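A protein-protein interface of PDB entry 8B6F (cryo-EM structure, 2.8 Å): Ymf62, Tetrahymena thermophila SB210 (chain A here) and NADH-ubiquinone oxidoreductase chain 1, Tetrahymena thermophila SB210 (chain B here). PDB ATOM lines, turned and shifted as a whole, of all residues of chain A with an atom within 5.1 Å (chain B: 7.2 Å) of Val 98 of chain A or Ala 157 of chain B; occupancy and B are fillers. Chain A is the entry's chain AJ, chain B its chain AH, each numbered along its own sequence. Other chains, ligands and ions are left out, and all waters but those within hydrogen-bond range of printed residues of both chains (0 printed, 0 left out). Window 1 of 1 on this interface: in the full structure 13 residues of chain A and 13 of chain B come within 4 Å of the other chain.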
ATOM      1  N   PHE A  94      15.016  -5.614  12.153  1.00  0.00           N
ATOM      2  CA  PHE A  94      15.142  -5.562  13.606  1.00  0.00           C
ATOM      3  C   PHE A  94      14.206  -6.566  14.269  1.00  0.00           C
ATOM      4  O   PHE A  94      14.611  -7.316  15.163  1.00  0.00           O
ATOM      5  CB  PHE A  94      14.843  -4.141  14.087  1.00  0.00           C
ATOM      6  CG  PHE A  94      15.456  -3.800  15.410  1.00  0.00           C
ATOM      7  CD1 PHE A  94      14.852  -4.196  16.589  1.00  0.00           C
ATOM      8  CD2 PHE A  94      16.620  -3.056  15.474  1.00  0.00           C
ATOM      9  CE1 PHE A  94      15.409  -3.873  17.807  1.00  0.00           C
ATOM     10  CE2 PHE A  94      17.182  -2.728  16.690  1.00  0.00           C
ATOM     11  CZ  PHE A  94      16.576  -3.137  17.858  1.00  0.00           C
ATOM     12  N   ILE A  95      12.946  -6.598  13.834  1.00  0.00           N
ATOM     13  CA  ILE A  95      11.981  -7.539  14.396  1.00  0.00           C
ATOM     14  C   ILE A  95      12.396  -8.971  14.088  1.00  0.00           C
ATOM     15  O   ILE A  95      12.192  -9.882  14.898  1.00  0.00           O
ATOM     16  CB  ILE A  95      10.567  -7.230  13.874  1.00  0.00           C
ATOM     17  CG1 ILE A  95      10.124  -5.845  14.352  1.00  0.00           C
ATOM     18  CG2 ILE A  95       9.577  -8.299  14.332  1.00  0.00           C
ATOM     19  CD1 ILE A  95       8.846  -5.351  13.715  1.00  0.00           C
ATOM     20  N   ALA A  96      12.981  -9.191  12.911  1.00  0.00           N
ATOM     21  CA  ALA A  96      13.472 -10.520  12.561  1.00  0.00           C
ATOM     22  C   ALA A  96      14.608 -10.949  13.480  1.00  0.00           C
ATOM     23  O   ALA A  96      14.687 -12.118  13.873  1.00  0.00           O
ATOM     24  CB  ALA A  96      13.926 -10.539  11.103  1.00  0.00           C
ATOM     25  N   VAL A  97      15.496 -10.022  13.838  1.00  0.00           N
ATOM     26  CA  VAL A  97      16.565 -10.352  14.776  1.00  0.00           C
ATOM     27  C   VAL A  97      15.980 -10.740  16.127  1.00  0.00           C
ATOM     28  O   VAL A  97      16.425 -11.706  16.757  1.00  0.00           O
ATOM     29  CB  VAL A  97      17.550  -9.174  14.900  1.00  0.00           C
ATOM     30  CG1 VAL A  97      18.520  -9.393  16.053  1.00  0.00           C
ATOM     31  CG2 VAL A  97      18.312  -8.982  13.604  1.00  0.00           C
ATOM     32  N   VAL A  98      14.976 -10.000  16.595  1.00  0.00           N
ATOM     33  CA  VAL A  98      14.332 -10.346  17.859  1.00  0.00           C
ATOM     34  C   VAL A  98      13.694 -11.725  17.762  1.00  0.00           C
ATOM     35  O   VAL A  98      13.767 -12.527  18.700  1.00  0.00           O
ATOM     36  CB  VAL A  98      13.303  -9.269  18.248  1.00  0.00           C
ATOM     37  CG1 VAL A  98      12.569  -9.659  19.524  1.00  0.00           C
ATOM     38  CG2 VAL A  98      13.988  -7.923  18.419  1.00  0.00           C
ATOM     39  N   LEU A  99      13.049 -12.019  16.632  1.00  0.00           N
ATOM     40  CA  LEU A  99      12.434 -13.329  16.450  1.00  0.00           C
ATOM     41  C   LEU A  99      13.484 -14.434  16.462  1.00  0.00           C
ATOM     42  O   LEU A  99      13.246 -15.522  16.997  1.00  0.00           O
ATOM     43  CB  LEU A  99      11.637 -13.352  15.146  1.00  0.00           C
ATOM     44  CG  LEU A  99      10.897 -14.648  14.812  1.00  0.00           C
ATOM     45  CD1 LEU A  99       9.867 -14.982  15.878  1.00  0.00           C
ATOM     46  CD2 LEU A  99      10.238 -14.542  13.449  1.00  0.00           C
ATOM     47  N   LEU A 100      14.651 -14.175  15.868  1.00  0.00           N
ATOM     48  CA  LEU A 100      15.730 -15.155  15.903  1.00  0.00           C
ATOM     49  C   LEU A 100      16.259 -15.347  17.318  1.00  0.00           C
ATOM     50  O   LEU A 100      16.620 -16.464  17.705  1.00  0.00           O
ATOM     51  CB  LEU A 100      16.861 -14.734  14.965  1.00  0.00           C
ATOM     52  CG  LEU A 100      16.566 -14.778  13.465  1.00  0.00           C
ATOM     53  CD1 LEU A 100      17.778 -14.311  12.685  1.00  0.00           C
ATOM     54  CD2 LEU A 100      16.150 -16.170  13.018  1.00  0.00           C
ATOM     55  N   PHE A 101      16.332 -14.273  18.104  1.00  0.00           N
ATOM     56  CA  PHE A 101      16.702 -14.431  19.505  1.00  0.00           C
ATOM     57  C   PHE A 101      15.702 -15.325  20.227  1.00  0.00           C
ATOM     58  O   PHE A 101      16.088 -16.171  21.040  1.00  0.00           O
ATOM     59  CB  PHE A 101      16.782 -13.065  20.190  1.00  0.00           C
ATOM     60  CG  PHE A 101      17.914 -12.194  19.711  1.00  0.00           C
ATOM     61  CD1 PHE A 101      18.934 -12.706  18.926  1.00  0.00           C
ATOM     62  CD2 PHE A 101      17.956 -10.855  20.057  1.00  0.00           C
ATOM     63  CE1 PHE A 101      19.967 -11.898  18.495  1.00  0.00           C
ATOM     64  CE2 PHE A 101      18.986 -10.044  19.629  1.00  0.00           C
ATOM     65  CZ  PHE A 101      19.991 -10.565  18.847  1.00  0.00           C
ATOM     66  N   TYR A 102      14.410 -15.147  19.947  1.00  0.00           N
ATOM     67  CA  TYR A 102      13.395 -15.963  20.602  1.00  0.00           C
ATOM     68  C   TYR A 102      13.502 -17.422  20.180  1.00  0.00           C
ATOM     69  O   TYR A 102      13.544 -18.323  21.025  1.00  0.00           O
ATOM     70  CB  TYR A 102      12.005 -15.417  20.280  1.00  0.00           C
ATOM     71  CG  TYR A 102      10.880 -16.229  20.879  1.00  0.00           C
ATOM     72  CD1 TYR A 102      10.970 -16.728  22.172  1.00  0.00           C
ATOM     73  CD2 TYR A 102       9.724 -16.488  20.156  1.00  0.00           C
ATOM     74  CE1 TYR A 102       9.945 -17.466  22.726  1.00  0.00           C
ATOM     75  CE2 TYR A 102       8.692 -17.225  20.701  1.00  0.00           C
ATOM     76  CZ  TYR A 102       8.809 -17.711  21.987  1.00  0.00           C
ATOM     77  OH  TYR A 102       7.785 -18.444  22.533  1.00  0.00           O
ATOM     78  N   SER B 134      20.814   1.115  17.098  1.00  0.00           N
ATOM     79  CA  SER B 134      20.091   0.130  17.892  1.00  0.00           C
ATOM     80  C   SER B 134      20.456  -1.285  17.460  1.00  0.00           C
ATOM     81  O   SER B 134      20.609  -2.177  18.301  1.00  0.00           O
ATOM     82  CB  SER B 134      18.585   0.360  17.775  1.00  0.00           C
ATOM     83  OG  SER B 134      18.151   0.218  16.434  1.00  0.00           O
ATOM     84  N   ILE B 137      23.732  -2.046  19.121  1.00  0.00           N
ATOM     85  CA  ILE B 137      23.584  -2.324  20.545  1.00  0.00           C
ATOM     86  C   ILE B 137      23.037  -3.731  20.754  1.00  0.00           C
ATOM     87  O   ILE B 137      23.519  -4.475  21.615  1.00  0.00           O
ATOM     88  CB  ILE B 137      22.690  -1.260  21.206  1.00  0.00           C
ATOM     89  CG1 ILE B 137      23.435   0.075  21.283  1.00  0.00           C
ATOM     90  CG2 ILE B 137      22.245  -1.712  22.597  1.00  0.00           C
ATOM     91  CD1 ILE B 137      22.585   1.230  21.767  1.00  0.00           C
ATOM     92  N   MET B 138      22.020  -4.115  19.982  1.00  0.00           N
ATOM     93  CA  MET B 138      21.463  -5.456  20.125  1.00  0.00           C
ATOM     94  C   MET B 138      22.506  -6.521  19.817  1.00  0.00           C
ATOM     95  O   MET B 138      22.618  -7.520  20.535  1.00  0.00           O
ATOM     96  CB  MET B 138      20.260  -5.634  19.205  1.00  0.00           C
ATOM     97  CG  MET B 138      18.967  -5.066  19.738  1.00  0.00           C
ATOM     98  SD  MET B 138      17.552  -6.051  19.212  1.00  0.00           S
ATOM     99  CE  MET B 138      17.868  -6.225  17.457  1.00  0.00           C
ATOM    100  N   PHE B 150      22.362  -9.518  27.395  1.00  0.00           N
ATOM    101  CA  PHE B 150      21.297  -9.944  26.499  1.00  0.00           C
ATOM    102  C   PHE B 150      19.959  -9.346  26.915  1.00  0.00           C
ATOM    103  O   PHE B 150      19.172  -8.924  26.061  1.00  0.00           O
ATOM    104  CB  PHE B 150      21.232 -11.471  26.456  1.00  0.00           C
ATOM    105  CG  PHE B 150      20.528 -12.012  25.248  1.00  0.00           C
ATOM    106  CD1 PHE B 150      20.847 -11.555  23.980  1.00  0.00           C
ATOM    107  CD2 PHE B 150      19.570 -12.999  25.372  1.00  0.00           C
ATOM    108  CE1 PHE B 150      20.211 -12.054  22.869  1.00  0.00           C
ATOM    109  CE2 PHE B 150      18.930 -13.502  24.259  1.00  0.00           C
ATOM    110  CZ  PHE B 150      19.252 -13.030  23.008  1.00  0.00           C
ATOM    111  N   MET B 151      19.684  -9.295  28.219  1.00  0.00           N
ATOM    112  CA  MET B 151      18.466  -8.636  28.684  1.00  0.00           C
ATOM    113  C   MET B 151      18.486  -7.153  28.340  1.00  0.00           C
ATOM    114  O   MET B 151      17.452  -6.575  27.987  1.00  0.00           O
ATOM    115  CB  MET B 151      18.294  -8.839  30.188  1.00  0.00           C
ATOM    116  CG  MET B 151      17.908 -10.260  30.567  1.00  0.00           C
ATOM    117  SD  MET B 151      17.562 -10.469  32.324  1.00  0.00           S
ATOM    118  CE  MET B 151      19.171 -10.145  33.039  1.00  0.00           C
ATOM    119  N   ALA B 152      19.656  -6.521  28.428  1.00  0.00           N
ATOM    120  CA  ALA B 152      19.780  -5.127  28.018  1.00  0.00           C
ATOM    121  C   ALA B 152      19.478  -4.962  26.535  1.00  0.00           C
ATOM    122  O   ALA B 152      18.859  -3.973  26.126  1.00  0.00           O
ATOM    123  CB  ALA B 152      21.181  -4.608  28.335  1.00  0.00           C
ATOM    124  N   SER B 153      19.915  -5.915  25.711  1.00  0.00           N
ATOM    125  CA  SER B 153      19.612  -5.852  24.286  1.00  0.00           C
ATOM    126  C   SER B 153      18.115  -5.974  24.036  1.00  0.00           C
ATOM    127  O   SER B 153      17.567  -5.279  23.172  1.00  0.00           O
ATOM    128  CB  SER B 153      20.369  -6.951  23.542  1.00  0.00           C
ATOM    129  OG  SER B 153      19.838  -8.229  23.840  1.00  0.00           O
ATOM    130  N   ILE B 154      17.435  -6.853  24.773  1.00  0.00           N
ATOM    131  CA  ILE B 154      15.987  -6.975  24.624  1.00  0.00           C
ATOM    132  C   ILE B 154      15.306  -5.681  25.046  1.00  0.00           C
ATOM    133  O   ILE B 154      14.353  -5.225  24.403  1.00  0.00           O
ATOM    134  CB  ILE B 154      15.466  -8.184  25.422  1.00  0.00           C
ATOM    135  CG1 ILE B 154      16.116  -9.478  24.923  1.00  0.00           C
ATOM    136  CG2 ILE B 154      13.948  -8.281  25.325  1.00  0.00           C
ATOM    137  CD1 ILE B 154      15.896  -9.772  23.449  1.00  0.00           C
ATOM    138  N   ARG B 155      15.779  -5.068  26.132  1.00  0.00           N
ATOM    139  CA  ARG B 155      15.240  -3.777  26.544  1.00  0.00           C
ATOM    140  C   ARG B 155      15.473  -2.728  25.468  1.00  0.00           C
ATOM    141  O   ARG B 155      14.606  -1.886  25.211  1.00  0.00           O
ATOM    142  CB  ARG B 155      15.868  -3.330  27.862  1.00  0.00           C
ATOM    143  CG  ARG B 155      15.451  -4.157  29.057  1.00  0.00           C
ATOM    144  CD  ARG B 155      16.028  -3.579  30.329  1.00  0.00           C
ATOM    145  NE  ARG B 155      15.565  -4.295  31.509  1.00  0.00           N
ATOM    146  CZ  ARG B 155      15.829  -3.930  32.754  1.00  0.00           C
ATOM    147  NH1 ARG B 155      16.551  -2.854  33.020  1.00  0.00           N
ATOM    148  NH2 ARG B 155      15.359  -4.662  33.760  1.00  0.00           N
ATOM    149  N   CYS B 156      16.643  -2.763  24.830  1.00  0.00           N
ATOM    150  CA  CYS B 156      16.903  -1.853  23.721  1.00  0.00           C
ATOM    151  C   CYS B 156      15.922  -2.091  22.585  1.00  0.00           C
ATOM    152  O   CYS B 156      15.457  -1.140  21.946  1.00  0.00           O
ATOM    153  CB  CYS B 156      18.338  -2.026  23.228  1.00  0.00           C
ATOM    154  SG  CYS B 156      18.658  -1.233  21.642  1.00  0.00           S
ATOM    155  N   ALA B 157      15.599  -3.355  22.310  1.00  0.00           N
ATOM    156  CA  ALA B 157      14.614  -3.649  21.277  1.00  0.00           C
ATOM    157  C   ALA B 157      13.259  -3.045  21.624  1.00  0.00           C
ATOM    158  O   ALA B 157      12.605  -2.440  20.768  1.00  0.00           O
ATOM    159  CB  ALA B 157      14.492  -5.159  21.086  1.00  0.00           C
ATOM    160  N   ILE B 158      12.827  -3.186  22.879  1.00  0.00           N
ATOM    161  CA  ILE B 158      11.545  -2.620  23.292  1.00  0.00           C
ATOM    162  C   ILE B 158      11.577  -1.102  23.172  1.00  0.00           C
ATOM    163  O   ILE B 158      10.613  -0.480  22.713  1.00  0.00           O
ATOM    164  CB  ILE B 158      11.198  -3.073  24.721  1.00  0.00           C
ATOM    165  CG1 ILE B 158      11.089  -4.599  24.777  1.00  0.00           C
ATOM    166  CG2 ILE B 158       9.893  -2.438  25.178  1.00  0.00           C
ATOM    167  CD1 ILE B 158      11.013  -5.158  26.180  1.00  0.00           C
ATOM    168  N   LEU B 159      12.681  -0.481  23.588  1.00  0.00           N
ATOM    169  CA  LEU B 159      12.805   0.966  23.462  1.00  0.00           C
ATOM    170  C   LEU B 159      12.726   1.393  22.003  1.00  0.00           C
ATOM    171  O   LEU B 159      12.087   2.399  21.675  1.00  0.00           O
ATOM    172  CB  LEU B 159      14.115   1.444  24.085  1.00  0.00           C
ATOM    173  CG  LEU B 159      14.200   1.452  25.610  1.00  0.00           C
ATOM    174  CD1 LEU B 159      15.594   1.842  26.058  1.00  0.00           C
ATOM    175  CD2 LEU B 159      13.174   2.417  26.186  1.00  0.00           C
ATOM    176  N   MET B 160      13.370   0.638  21.115  1.00  0.00           N
ATOM    177  CA  MET B 160      13.298   0.946  19.692  1.00  0.00           C
ATOM    178  C   MET B 160      11.868   0.820  19.180  1.00  0.00           C
ATOM    179  O   MET B 160      11.407   1.659  18.397  1.00  0.00           O
ATOM    180  CB  MET B 160      14.236   0.019  18.919  1.00  0.00           C
ATOM    181  CG  MET B 160      14.637   0.525  17.540  1.00  0.00           C
ATOM    182  SD  MET B 160      13.310   0.513  16.319  1.00  0.00           S
ATOM    183  CE  MET B 160      12.878  -1.224  16.258  1.00  0.00           C
ATOM    184  N   LEU B 161      11.145  -0.211  19.619  1.00  0.00           N
ATOM    185  CA  LEU B 161       9.754  -0.366  19.204  1.00  0.00           C
ATOM    186  C   LEU B 161       8.932   0.854  19.601  1.00  0.00           C
ATOM    187  O   LEU B 161       8.160   1.388  18.796  1.00  0.00           O
ATOM    188  CB  LEU B 161       9.162  -1.632  19.827  1.00  0.00           C
ATOM    189  CG  LEU B 161       9.733  -2.975  19.364  1.00  0.00           C
ATOM    190  CD1 LEU B 161       9.146  -4.110  20.187  1.00  0.00           C
ATOM    191  CD2 LEU B 161       9.480  -3.210  17.888  1.00  0.00           C
ATOM    192  N   ASN B 162       9.082   1.309  20.846  1.00  0.00           N
ATOM    193  CA  ASN B 162       8.351   2.489  21.297  1.00  0.00           C
ATOM    194  C   ASN B 162       8.788   3.731  20.532  1.00  0.00           C
ATOM    195  O   ASN B 162       7.953   4.551  20.134  1.00  0.00           O
ATOM    196  CB  ASN B 162       8.553   2.693  22.797  1.00  0.00           C
ATOM    197  CG  ASN B 162       7.949   1.579  23.620  1.00  0.00           C
ATOM    198  OD1 ASN B 162       6.897   1.042  23.279  1.00  0.00           O
ATOM    199  ND2 ASN B 162       8.614   1.221  24.712  1.00  0.00           N
ATOM    200  N   ILE B 163      10.096   3.886  20.320  1.00  0.00           N
ATOM    201  CA  ILE B 163      10.610   5.076  19.649  1.00  0.00           C
ATOM    202  C   ILE B 163      10.047   5.185  18.241  1.00  0.00           C
ATOM    203  O   ILE B 163       9.721   6.284  17.774  1.00  0.00           O
ATOM    204  CB  ILE B 163      12.150   5.055  19.642  1.00  0.00           C
ATOM    205  CG1 ILE B 163      12.685   5.363  21.039  1.00  0.00           C
ATOM    206  CG2 ILE B 163      12.710   6.053  18.630  1.00  0.00           C
ATOM    207  CD1 ILE B 163      14.157   5.072  21.211  1.00  0.00           C
ATOM    208  N   ALA B 222      18.267   0.387  28.698  1.00  0.00           N
ATOM    209  CA  ALA B 222      19.311  -0.456  28.126  1.00  0.00           C
ATOM    210  C   ALA B 222      20.570  -0.435  28.981  1.00  0.00           C
ATOM    211  O   ALA B 222      21.207  -1.475  29.187  1.00  0.00           O
ATOM    212  CB  ALA B 222      19.627  -0.004  26.701  1.00  0.00           C
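The backbone carbonyl oxygen of Phe 150 of chain B sits at hydrogen-bond distance from the side-chain hydroxyl of Ser 153 of chain B (2.4 Å).
Phe 94 of chain A touches Ser 134 of chain B.
Met 138 of chain B touches Phe 94 of chain A.
Ala 157 of chain B touches Phe 94 of chain A.
CE of Met 160 of chain B touches CD1 of Phe 94 of chain A, 3.6 Å away.
Val 97 of chain A touches Met 138 of chain B.
Val 98 of chain A touches Ala 157 of chain B (CG2 to CB, 3.9 Å).
Phe 101 of chain A touches Phe 150 of chain B.
Of the printed residues of chain B, Phe 94 of chain A touches Ser 134 (3.1 Å), Met 138 (3.4 Å), Ala 157 (3.6 Å) and Met 160 (3.6 Å).
Val 98 of chain A touches just one residue of chain B: Ala 157.
Printed residues of chain B within 4 Å of Phe 101 of chain A: Phe 150 (3.7 Å).
Printed residues of chain A within 4 Å of Ser 134 of chain B: Phe 94 (3.1 Å).
Ala 157 of chain B touches just these residues of chain A: Phe 94 and Val 98.
Printed residues of chain A within 4 Å of Met 160 of chain B: Phe 94.
The nearest residue of chain B that does not touch Val 98 of chain A is Met 138 of chain B (4.1 Å).
Hydrophobic or aromatic side chains of chain B within 4 Å of the printed part of chain A: Met 138, Phe 150, Ala 157 and Met 160.
Of the 9 printed residues of chain A, 4 touch a printed residue of chain B.
Printed residues of chain A that touch a printed residue of chain B: Phe 94, Val 97, Val 98 and Phe 101.
Hydrophobic or aromatic side chains of chain A that line the printed part of chain B: Phe 94, Val 97, Val 98 and Phe 101.
Among the printed residues, no Asp or Glu carboxylate lies within 4 Å of a Lys or Arg side-chain nitrogen of the other chain.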
